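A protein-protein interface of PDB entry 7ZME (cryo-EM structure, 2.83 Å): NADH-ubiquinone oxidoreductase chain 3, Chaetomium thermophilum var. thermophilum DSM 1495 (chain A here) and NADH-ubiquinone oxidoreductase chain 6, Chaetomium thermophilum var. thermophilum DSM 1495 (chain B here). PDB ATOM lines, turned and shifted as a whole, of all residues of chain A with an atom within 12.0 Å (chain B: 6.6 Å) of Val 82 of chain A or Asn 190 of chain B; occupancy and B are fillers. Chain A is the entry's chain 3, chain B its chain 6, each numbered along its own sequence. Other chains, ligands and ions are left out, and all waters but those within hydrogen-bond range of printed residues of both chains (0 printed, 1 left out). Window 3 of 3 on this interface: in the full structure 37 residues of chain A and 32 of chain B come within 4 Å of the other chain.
Among the printed residues, pairs that only touch across the chains: Leu 72 of chain A with Met 192 of chain B (3.5 Å), Leu 73 of chain A with Tyr 193 of chain B (3.7 Å), Tyr 74 of chain A with Ile 185 of chain B (3.9 Å), Pro 75 of chain A with Ile 185 of chain B (3.7 Å), Pro 75 of chain A with Gly 189 of chain B (3.8 Å), Pro 75 of chain A with Met 192 of chain B (3.8 Å), Pro 75 of chain A with Tyr 193 of chain B (3.5 Å), Val 78 of chain A with Ile 185 of chain B (3.6 Å), Ser 79 of chain A with Ser 186 of chain B (3.7 Å), Val 82 of chain A with Asn 190 of chain B (3.6 Å), Asn 83 of chain A with Tyr 193 of chain B (3.7 Å), Tyr 86 of chain A with Thr 194 of chain B (3.5 Å), Gly 87 of chain A with Tyr 193 of chain B (3.8 Å), Gly 87 of chain A with Thr 194 of chain B (3.8 Å) and Ala 90 of chain A with Tyr 193 of chain B (3.2 Å).
Hydrophobic or aromatic side chains of chain B within 4 Å of the printed part of chain A: Ile 185, Met 192 and Tyr 193. Of the 21 printed residues of chain A, 12 touch a printed residue of chain B. Hydrophobic or aromatic side chains of chain A that line the printed part of chain B: Leu 72, Pro 75, Phe 76, Val 78, Val 82, Tyr 86 and Ala 90.
OH of Tyr 193 of chain B lies within hydrogen-bond range of O of Leu 72 of chain A, at 2.6 Å. N of Phe 76 of chain A lies within hydrogen-bond range of OH of Tyr 193 of chain B (3.0 Å). The backbone carbonyl oxygen of Val 78 of chain A is in hydrogen-bond range of the side-chain hydroxyl of Ser 186 of chain B, at 2.9 Å. OG of Ser 79 of chain A lies close to O of Gly 189 of chain B, at 3.4 Å. The side-chain amide nitrogen (ND2) of Asn 190 of chain B lies within hydrogen-bond range of the side-chain hydroxyl (OG) of Ser 79 of chain A, 2.7 Å away. The side-chain amide nitrogen (ND2) of Asn 83 of chain A is in hydrogen-bond range of the backbone carbonyl oxygen (O) of Gly 189 of chain B, 3.1 Å away.
ND2 of Asn 83 of chain A sits at hydrogen-bond distance from O of Ser 79 of chain A, 3.0 Å away. The side-chain amide nitrogen of Asn 182 of chain B lies within hydrogen-bond range of the side-chain amide oxygen of Asn 190 of chain B. The backbone carbonyl oxygen (O) of Ser 186 of chain B lies within hydrogen-bond range of the side-chain amide nitrogen (ND2) of Asn 190 of chain B, 3.2 Å away. The backbone carbonyl oxygen (O) of Asn 190 of chain B sits at hydrogen-bond distance from the side-chain hydroxyl (OG1) of Thr 194 of chain B (3.4 Å). OH of Tyr 193 of chain B lies within hydrogen-bond range of SD of Met 192 of chain B (3.4 Å). OG1 of Thr 194 of chain B lies within hydrogen-bond range of OD1 of Asn 195 of chain B, at 2.8 Å.
Val 82 of chain A touches just one residue of chain B: Asn 190. Of the printed residues of chain B, Gly 87 of chain A touches Tyr 193 (3.8 Å) and Thr 194 (3.8 Å). No residue of chain A comes within 4 Å of Asn 182 of chain B. Gly 189 of chain B touches just these residues of chain A: Pro 75, Ser 79 and Asn 83. No residue of chain A comes within 4 Å of Ile 191 of chain B. Printed residues of chain A within 4 Å of Met 192 of chain B: Leu 72 and Pro 75. The nearest residue of chain A that does not touch Asn 190 of chain B is Asn 83 of chain A (4.4 Å).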
ATOM      1  N   LEU A  71      29.250 -29.230  39.133  1.00  0.00           N
ATOM      2  CA  LEU A  71      30.130 -28.390  38.327  1.00  0.00           C
ATOM      3  C   LEU A  71      30.282 -28.942  36.916  1.00  0.00           C
ATOM      4  O   LEU A  71      30.399 -28.171  35.957  1.00  0.00           O
ATOM      5  CB  LEU A  71      31.500 -28.258  38.992  1.00  0.00           C
ATOM      6  CG  LEU A  71      32.405 -27.179  38.382  1.00  0.00           C
ATOM      7  CD1 LEU A  71      32.003 -25.794  38.871  1.00  0.00           C
ATOM      8  CD2 LEU A  71      33.877 -27.446  38.656  1.00  0.00           C
ATOM      9  N   LEU A  72      30.292 -30.265  36.765  1.00  0.00           N
ATOM     10  CA  LEU A  72      30.390 -30.888  35.452  1.00  0.00           C
ATOM     11  C   LEU A  72      29.081 -30.845  34.682  1.00  0.00           C
ATOM     12  O   LEU A  72      29.011 -31.398  33.580  1.00  0.00           O
ATOM     13  CB  LEU A  72      30.850 -32.343  35.568  1.00  0.00           C
ATOM     14  CG  LEU A  72      32.289 -32.678  35.960  1.00  0.00           C
ATOM     15  CD1 LEU A  72      32.553 -34.144  35.697  1.00  0.00           C
ATOM     16  CD2 LEU A  72      33.306 -31.815  35.246  1.00  0.00           C
ATOM     17  N   LEU A  73      28.043 -30.224  35.241  1.00  0.00           N
ATOM     18  CA  LEU A  73      26.778 -30.035  34.549  1.00  0.00           C
ATOM     19  C   LEU A  73      26.542 -28.598  34.122  1.00  0.00           C
ATOM     20  O   LEU A  73      25.732 -28.365  33.223  1.00  0.00           O
ATOM     21  CB  LEU A  73      25.611 -30.485  35.439  1.00  0.00           C
ATOM     22  CG  LEU A  73      25.423 -31.992  35.593  1.00  0.00           C
ATOM     23  CD1 LEU A  73      24.491 -32.298  36.741  1.00  0.00           C
ATOM     24  CD2 LEU A  73      24.905 -32.596  34.304  1.00  0.00           C
ATOM     25  N   TYR A  74      27.225 -27.639  34.743  1.00  0.00           N
ATOM     26  CA  TYR A  74      27.079 -26.241  34.354  1.00  0.00           C
ATOM     27  C   TYR A  74      27.459 -25.964  32.905  1.00  0.00           C
ATOM     28  O   TYR A  74      26.773 -25.146  32.268  1.00  0.00           O
ATOM     29  CB  TYR A  74      27.880 -25.355  35.316  1.00  0.00           C
ATOM     30  CG  TYR A  74      27.046 -24.795  36.441  1.00  0.00           C
ATOM     31  CD1 TYR A  74      26.714 -25.574  37.537  1.00  0.00           C
ATOM     32  CD2 TYR A  74      26.579 -23.493  36.401  1.00  0.00           C
ATOM     33  CE1 TYR A  74      25.949 -25.069  38.563  1.00  0.00           C
ATOM     34  CE2 TYR A  74      25.812 -22.981  37.423  1.00  0.00           C
ATOM     35  CZ  TYR A  74      25.501 -23.772  38.501  1.00  0.00           C
ATOM     36  OH  TYR A  74      24.737 -23.260  39.520  1.00  0.00           O
ATOM     37  N   PRO A  75      28.517 -26.552  32.332  1.00  0.00           N
ATOM     38  CA  PRO A  75      28.732 -26.375  30.887  1.00  0.00           C
ATOM     39  C   PRO A  75      27.571 -26.852  30.034  1.00  0.00           C
ATOM     40  O   PRO A  75      27.332 -26.281  28.966  1.00  0.00           O
ATOM     41  CB  PRO A  75      30.001 -27.197  30.626  1.00  0.00           C
ATOM     42  CG  PRO A  75      30.725 -27.159  31.907  1.00  0.00           C
ATOM     43  CD  PRO A  75      29.669 -27.227  32.962  1.00  0.00           C
ATOM     44  N   PHE A  76      26.848 -27.889  30.460  1.00  0.00           N
ATOM     45  CA  PHE A  76      25.716 -28.361  29.671  1.00  0.00           C
ATOM     46  C   PHE A  76      24.585 -27.343  29.657  1.00  0.00           C
ATOM     47  O   PHE A  76      23.929 -27.152  28.627  1.00  0.00           O
ATOM     48  CB  PHE A  76      25.210 -29.701  30.203  1.00  0.00           C
ATOM     49  CG  PHE A  76      24.020 -30.224  29.459  1.00  0.00           C
ATOM     50  CD1 PHE A  76      24.184 -30.928  28.282  1.00  0.00           C
ATOM     51  CD2 PHE A  76      22.736 -29.998  29.929  1.00  0.00           C
ATOM     52  CE1 PHE A  76      23.090 -31.396  27.588  1.00  0.00           C
ATOM     53  CE2 PHE A  76      21.641 -30.463  29.237  1.00  0.00           C
ATOM     54  CZ  PHE A  76      21.818 -31.165  28.067  1.00  0.00           C
ATOM     55  N   ALA A  77      24.319 -26.690  30.787  1.00  0.00           N
ATOM     56  CA  ALA A  77      23.155 -25.777  30.853  1.00  0.00           C
ATOM     57  C   ALA A  77      23.388 -24.550  29.976  1.00  0.00           C
ATOM     58  O   ALA A  77      22.400 -23.944  29.543  1.00  0.00           O
ATOM     59  CB  ALA A  77      22.910 -25.400  32.280  1.00  0.00           C
ATOM     60  N   VAL A  78      24.653 -24.238  29.690  1.00  0.00           N
ATOM     61  CA  VAL A  78      25.002 -23.053  28.857  1.00  0.00           C
ATOM     62  C   VAL A  78      25.369 -23.494  27.437  1.00  0.00           C
ATOM     63  O   VAL A  78      25.855 -22.657  26.680  1.00  0.00           O
ATOM     64  CB  VAL A  78      26.108 -22.203  29.513  1.00  0.00           C
ATOM     65  CG1 VAL A  78      25.640 -21.551  30.798  1.00  0.00           C
ATOM     66  CG2 VAL A  78      27.391 -22.982  29.725  1.00  0.00           C
ATOM     67  N   SER A  79      25.175 -24.769  27.112  1.00  0.00           N
ATOM     68  CA  SER A  79      25.503 -25.279  25.757  1.00  0.00           C
ATOM     69  C   SER A  79      24.392 -26.180  25.223  1.00  0.00           C
ATOM     70  O   SER A  79      24.692 -27.029  24.395  1.00  0.00           O
ATOM     71  CB  SER A  79      26.815 -26.000  25.761  1.00  0.00           C
ATOM     72  OG  SER A  79      27.154 -26.450  24.461  1.00  0.00           O
ATOM     73  N   GLU A  80      23.153 -25.986  25.664  1.00  0.00           N
ATOM     74  CA  GLU A  80      22.064 -26.917  25.246  1.00  0.00           C
ATOM     75  C   GLU A  80      21.701 -26.829  23.757  1.00  0.00           C
ATOM     76  O   GLU A  80      21.300 -27.855  23.211  1.00  0.00           O
ATOM     77  CB  GLU A  80      20.842 -26.745  26.146  1.00  0.00           C
ATOM     78  CG  GLU A  80      20.962 -27.441  27.480  1.00  0.00           C
ATOM     79  CD  GLU A  80      20.059 -26.848  28.542  1.00  0.00           C
ATOM     80  OE1 GLU A  80      19.852 -27.509  29.571  1.00  0.00           O
ATOM     81  OE2 GLU A  80      19.576 -25.719  28.336  1.00  0.00           O
ATOM     82  N   TYR A  81      21.763 -25.656  23.131  1.00  0.00           N
ATOM     83  CA  TYR A  81      21.304 -25.538  21.721  1.00  0.00           C
ATOM     84  C   TYR A  81      22.186 -26.393  20.807  1.00  0.00           C
ATOM     85  O   TYR A  81      21.662 -27.026  19.885  1.00  0.00           O
ATOM     86  CB  TYR A  81      21.201 -24.070  21.303  1.00  0.00           C
ATOM     87  CG  TYR A  81      20.465 -23.835  20.013  1.00  0.00           C
ATOM     88  CD1 TYR A  81      19.082 -23.833  19.978  1.00  0.00           C
ATOM     89  CD2 TYR A  81      21.148 -23.624  18.827  1.00  0.00           C
ATOM     90  CE1 TYR A  81      18.393 -23.628  18.797  1.00  0.00           C
ATOM     91  CE2 TYR A  81      20.474 -23.418  17.637  1.00  0.00           C
ATOM     92  CZ  TYR A  81      19.091 -23.420  17.623  1.00  0.00           C
ATOM     93  OH  TYR A  81      18.415 -23.212  16.460  1.00  0.00           O
ATOM     94  N   VAL A  82      23.484 -26.421  21.084  1.00  0.00           N
ATOM     95  CA  VAL A  82      24.437 -27.197  20.248  1.00  0.00           C
ATOM     96  C   VAL A  82      24.394 -28.667  20.673  1.00  0.00           C
ATOM     97  O   VAL A  82      24.414 -29.531  19.784  1.00  0.00           O
ATOM     98  CB  VAL A  82      25.847 -26.591  20.342  1.00  0.00           C
ATOM     99  CG1 VAL A  82      26.927 -27.534  19.837  1.00  0.00           C
ATOM    100  CG2 VAL A  82      25.922 -25.245  19.642  1.00  0.00           C
ATOM    101  N   ASN A  83      24.306 -28.937  21.974  1.00  0.00           N
ATOM    102  CA  ASN A  83      24.351 -30.340  22.454  1.00  0.00           C
ATOM    103  C   ASN A  83      23.160 -31.124  21.906  1.00  0.00           C
ATOM    104  O   ASN A  83      23.386 -32.251  21.432  1.00  0.00           O
ATOM    105  CB  ASN A  83      24.436 -30.399  23.979  1.00  0.00           C
ATOM    106  CG  ASN A  83      25.855 -30.362  24.500  1.00  0.00           C
ATOM    107  OD1 ASN A  83      26.704 -31.121  24.047  1.00  0.00           O
ATOM    108  ND2 ASN A  83      26.114 -29.496  25.464  1.00  0.00           N
ATOM    109  N   SER A  84      21.951 -30.561  21.970  1.00  0.00           N
ATOM    110  CA  SER A  84      20.729 -31.201  21.412  1.00  0.00           C
ATOM    111  C   SER A  84      20.491 -32.587  22.013  1.00  0.00           C
ATOM    112  O   SER A  84      20.804 -32.766  23.192  1.00  0.00           O
ATOM    113  CB  SER A  84      20.727 -31.209  19.911  1.00  0.00           C
ATOM    114  OG  SER A  84      19.467 -31.612  19.402  1.00  0.00           O
ATOM    115  N   ALA A  85      19.928 -33.514  21.233  1.00  0.00           N
ATOM    116  CA  ALA A  85      19.630 -34.885  21.704  1.00  0.00           C
ATOM    117  C   ALA A  85      20.901 -35.684  21.988  1.00  0.00           C
ATOM    118  O   ALA A  85      20.964 -36.337  23.031  1.00  0.00           O
ATOM    119  CB  ALA A  85      18.810 -35.583  20.655  1.00  0.00           C
ATOM    120  N   TYR A  86      21.883 -35.615  21.099  1.00  0.00           N
ATOM    121  CA  TYR A  86      23.082 -36.464  21.267  1.00  0.00           C
ATOM    122  C   TYR A  86      23.834 -36.044  22.530  1.00  0.00           C
ATOM    123  O   TYR A  86      24.357 -36.917  23.243  1.00  0.00           O
ATOM    124  CB  TYR A  86      23.987 -36.389  20.037  1.00  0.00           C
ATOM    125  CG  TYR A  86      25.065 -37.438  20.049  1.00  0.00           C
ATOM    126  CD1 TYR A  86      24.748 -38.776  19.895  1.00  0.00           C
ATOM    127  CD2 TYR A  86      26.390 -37.102  20.255  1.00  0.00           C
ATOM    128  CE1 TYR A  86      25.724 -39.754  19.928  1.00  0.00           C
ATOM    129  CE2 TYR A  86      27.380 -38.066  20.289  1.00  0.00           C
ATOM    130  CZ  TYR A  86      27.043 -39.395  20.124  1.00  0.00           C
ATOM    131  OH  TYR A  86      28.008 -40.351  20.157  1.00  0.00           O
ATOM    132  N   GLY A  87      23.905 -34.736  22.775  1.00  0.00           N
ATOM    133  CA  GLY A  87      24.604 -34.300  23.968  1.00  0.00           C
ATOM    134  C   GLY A  87      23.783 -34.474  25.226  1.00  0.00           C
ATOM    135  O   GLY A  87      24.336 -34.690  26.306  1.00  0.00           O
ATOM    136  N   LEU A  88      22.456 -34.384  25.107  1.00  0.00           N
ATOM    137  CA  LEU A  88      21.580 -34.628  26.247  1.00  0.00           C
ATOM    138  C   LEU A  88      21.705 -36.063  26.737  1.00  0.00           C
ATOM    139  O   LEU A  88      21.652 -36.320  27.944  1.00  0.00           O
ATOM    140  CB  LEU A  88      20.132 -34.316  25.870  1.00  0.00           C
ATOM    141  CG  LEU A  88      19.034 -34.813  26.814  1.00  0.00           C
ATOM    142  CD1 LEU A  88      18.848 -33.870  27.984  1.00  0.00           C
ATOM    143  CD2 LEU A  88      17.732 -35.007  26.067  1.00  0.00           C
ATOM    144  N   ALA A  89      21.861 -37.012  25.813  1.00  0.00           N
ATOM    145  CA  ALA A  89      21.964 -38.417  26.194  1.00  0.00           C
ATOM    146  C   ALA A  89      23.172 -38.660  27.087  1.00  0.00           C
ATOM    147  O   ALA A  89      23.059 -39.282  28.147  1.00  0.00           O
ATOM    148  CB  ALA A  89      22.035 -39.290  24.945  1.00  0.00           C
ATOM    149  N   ALA A  90      24.342 -38.167  26.675  1.00  0.00           N
ATOM    150  CA  ALA A  90      25.544 -38.352  27.478  1.00  0.00           C
ATOM    151  C   ALA A  90      25.408 -37.678  28.836  1.00  0.00           C
ATOM    152  O   ALA A  90      25.831 -38.230  29.857  1.00  0.00           O
ATOM    153  CB  ALA A  90      26.759 -37.814  26.731  1.00  0.00           C
ATOM    154  N   ALA A  91      24.823 -36.478  28.863  1.00  0.00           N
ATOM    155  CA  ALA A  91      24.585 -35.793  30.126  1.00  0.00           C
ATOM    156  C   ALA A  91      23.612 -36.560  31.008  1.00  0.00           C
ATOM    157  O   ALA A  91      23.709 -36.494  32.237  1.00  0.00           O
ATOM    158  CB  ALA A  91      24.070 -34.379  29.865  1.00  0.00           C
ATOM    159  N   ASN B 182      31.437 -17.657  21.583  1.00  0.00           N
ATOM    160  CA  ASN B 182      30.872 -18.363  22.751  1.00  0.00           C
ATOM    161  C   ASN B 182      31.702 -17.994  23.968  1.00  0.00           C
ATOM    162  O   ASN B 182      32.838 -17.540  23.786  1.00  0.00           O
ATOM    163  CB  ASN B 182      30.903 -19.883  22.571  1.00  0.00           C
ATOM    164  CG  ASN B 182      30.041 -20.404  21.444  1.00  0.00           C
ATOM    165  OD1 ASN B 182      29.386 -19.637  20.750  1.00  0.00           O
ATOM    166  ND2 ASN B 182      30.035 -21.711  21.263  1.00  0.00           N
ATOM    167  N   ILE B 185      33.056 -21.484  28.858  1.00  0.00           N
ATOM    168  CA  ILE B 185      32.252 -22.590  29.453  1.00  0.00           C
ATOM    169  C   ILE B 185      31.366 -23.185  28.359  1.00  0.00           C
ATOM    170  O   ILE B 185      31.172 -24.410  28.375  1.00  0.00           O
ATOM    171  CB  ILE B 185      31.469 -22.087  30.683  1.00  0.00           C
ATOM    172  CG1 ILE B 185      30.644 -23.198  31.336  1.00  0.00           C
ATOM    173  CG2 ILE B 185      30.632 -20.857  30.359  1.00  0.00           C
ATOM    174  CD1 ILE B 185      29.812 -22.743  32.507  1.00  0.00           C
ATOM    175  N   SER B 186      30.816 -22.343  27.478  1.00  0.00           N
ATOM    176  CA  SER B 186      29.985 -22.817  26.346  1.00  0.00           C
ATOM    177  C   SER B 186      30.843 -23.599  25.347  1.00  0.00           C
ATOM    178  O   SER B 186      30.370 -24.614  24.840  1.00  0.00           O
ATOM    179  CB  SER B 186      29.268 -21.674  25.712  1.00  0.00           C
ATOM    180  OG  SER B 186      28.150 -22.138  24.975  1.00  0.00           O
ATOM    181  N   SER B 187      32.062 -23.142  25.094  1.00  0.00           N
ATOM    182  CA  SER B 187      32.985 -23.832  24.161  1.00  0.00           C
ATOM    183  C   SER B 187      33.332 -25.221  24.693  1.00  0.00           C
ATOM    184  O   SER B 187      33.445 -26.148  23.875  1.00  0.00           O
ATOM    185  CB  SER B 187      34.208 -23.008  23.921  1.00  0.00           C
ATOM    186  OG  SER B 187      33.855 -21.671  23.612  1.00  0.00           O
ATOM    187  N   ILE B 188      33.480 -25.354  26.009  1.00  0.00           N
ATOM    188  CA  ILE B 188      33.785 -26.664  26.630  1.00  0.00           C
ATOM    189  C   ILE B 188      32.495 -27.482  26.563  1.00  0.00           C
ATOM    190  O   ILE B 188      32.581 -28.650  26.179  1.00  0.00           O
ATOM    191  CB  ILE B 188      34.229 -26.451  28.086  1.00  0.00           C
ATOM    192  CG1 ILE B 188      35.588 -25.754  28.180  1.00  0.00           C
ATOM    193  CG2 ILE B 188      34.215 -27.756  28.867  1.00  0.00           C
ATOM    194  CD1 ILE B 188      35.901 -25.197  29.542  1.00  0.00           C
ATOM    195  N   GLY B 189      31.341 -26.865  26.810  1.00  0.00           N
ATOM    196  CA  GLY B 189      30.100 -27.609  26.701  1.00  0.00           C
ATOM    197  C   GLY B 189      29.817 -28.115  25.303  1.00  0.00           C
ATOM    198  O   GLY B 189      29.177 -29.155  25.134  1.00  0.00           O
ATOM    199  N   ASN B 190      30.285 -27.392  24.283  1.00  0.00           N
ATOM    200  CA  ASN B 190      30.080 -27.814  22.902  1.00  0.00           C
ATOM    201  C   ASN B 190      30.688 -29.180  22.613  1.00  0.00           C
ATOM    202  O   ASN B 190      30.230 -29.869  21.697  1.00  0.00           O
ATOM    203  CB  ASN B 190      30.671 -26.780  21.944  1.00  0.00           C
ATOM    204  CG  ASN B 190      29.829 -25.522  21.838  1.00  0.00           C
ATOM    205  OD1 ASN B 190      30.267 -24.518  21.281  1.00  0.00           O
ATOM    206  ND2 ASN B 190      28.618 -25.570  22.372  1.00  0.00           N
ATOM    207  N   ILE B 191      31.704 -29.584  23.373  1.00  0.00           N
ATOM    208  CA  ILE B 191      32.437 -30.818  23.099  1.00  0.00           C
ATOM    209  C   ILE B 191      32.495 -31.763  24.284  1.00  0.00           C
ATOM    210  O   ILE B 191      32.801 -32.954  24.105  1.00  0.00           O
ATOM    211  CB  ILE B 191      33.864 -30.483  22.624  1.00  0.00           C
ATOM    212  CG1 ILE B 191      34.576 -29.683  23.710  1.00  0.00           C
ATOM    213  CG2 ILE B 191      33.828 -29.705  21.328  1.00  0.00           C
ATOM    214  CD1 ILE B 191      36.031 -29.538  23.494  1.00  0.00           C
ATOM    215  N   MET B 192      32.222 -31.300  25.502  1.00  0.00           N
ATOM    216  CA  MET B 192      32.398 -32.112  26.698  1.00  0.00           C
ATOM    217  C   MET B 192      31.395 -33.256  26.783  1.00  0.00           C
ATOM    218  O   MET B 192      31.630 -34.224  27.515  1.00  0.00           O
ATOM    219  CB  MET B 192      32.304 -31.192  27.917  1.00  0.00           C
ATOM    220  CG  MET B 192      32.121 -31.842  29.260  1.00  0.00           C
ATOM    221  SD  MET B 192      31.773 -30.576  30.480  1.00  0.00           S
ATOM    222  CE  MET B 192      32.183 -31.445  31.976  1.00  0.00           C
ATOM    223  N   TYR B 193      30.295 -33.178  26.041  1.00  0.00           N
ATOM    224  CA  TYR B 193      29.231 -34.201  26.193  1.00  0.00           C
ATOM    225  C   TYR B 193      29.016 -34.934  24.873  1.00  0.00           C
ATOM    226  O   TYR B 193      28.075 -35.725  24.774  1.00  0.00           O
ATOM    227  CB  TYR B 193      27.942 -33.544  26.690  1.00  0.00           C
ATOM    228  CG  TYR B 193      28.093 -32.678  27.914  1.00  0.00           C
ATOM    229  CD1 TYR B 193      27.989 -33.213  29.183  1.00  0.00           C
ATOM    230  CD2 TYR B 193      28.338 -31.323  27.797  1.00  0.00           C
ATOM    231  CE1 TYR B 193      28.130 -32.426  30.312  1.00  0.00           C
ATOM    232  CE2 TYR B 193      28.489 -30.521  28.912  1.00  0.00           C
ATOM    233  CZ  TYR B 193      28.379 -31.074  30.173  1.00  0.00           C
ATOM    234  OH  TYR B 193      28.517 -30.282  31.272  1.00  0.00           O
ATOM    235  N   THR B 194      29.858 -34.664  23.882  1.00  0.00           N
ATOM    236  CA  THR B 194      29.772 -35.388  22.595  1.00  0.00           C
ATOM    237  C   THR B 194      31.162 -35.836  22.176  1.00  0.00           C
ATOM    238  O   THR B 194      31.452 -37.011  22.365  1.00  0.00           O
ATOM    239  CB  THR B 194      29.172 -34.507  21.494  1.00  0.00           C
ATOM    240  OG1 THR B 194      29.888 -33.275  21.409  1.00  0.00           O
ATOM    241  CG2 THR B 194      27.700 -34.223  21.702  1.00  0.00           C
ATOM    242  N   ASN B 195      32.011 -34.915  21.736  1.00  0.00           N
ATOM    243  CA  ASN B 195      33.342 -35.249  21.166  1.00  0.00           C
ATOM    244  C   ASN B 195      34.220 -35.960  22.195  1.00  0.00           C
ATOM    245  O   ASN B 195      34.978 -36.849  21.798  1.00  0.00           O
ATOM    246  CB  ASN B 195      34.011 -33.981  20.641  1.00  0.00           C
ATOM    247  CG  ASN B 195      33.192 -33.219  19.622  1.00  0.00           C
ATOM    248  OD1 ASN B 195      32.174 -32.619  19.950  1.00  0.00           O
ATOM    249  ND2 ASN B 195      33.646 -33.210  18.382  1.00  0.00           N
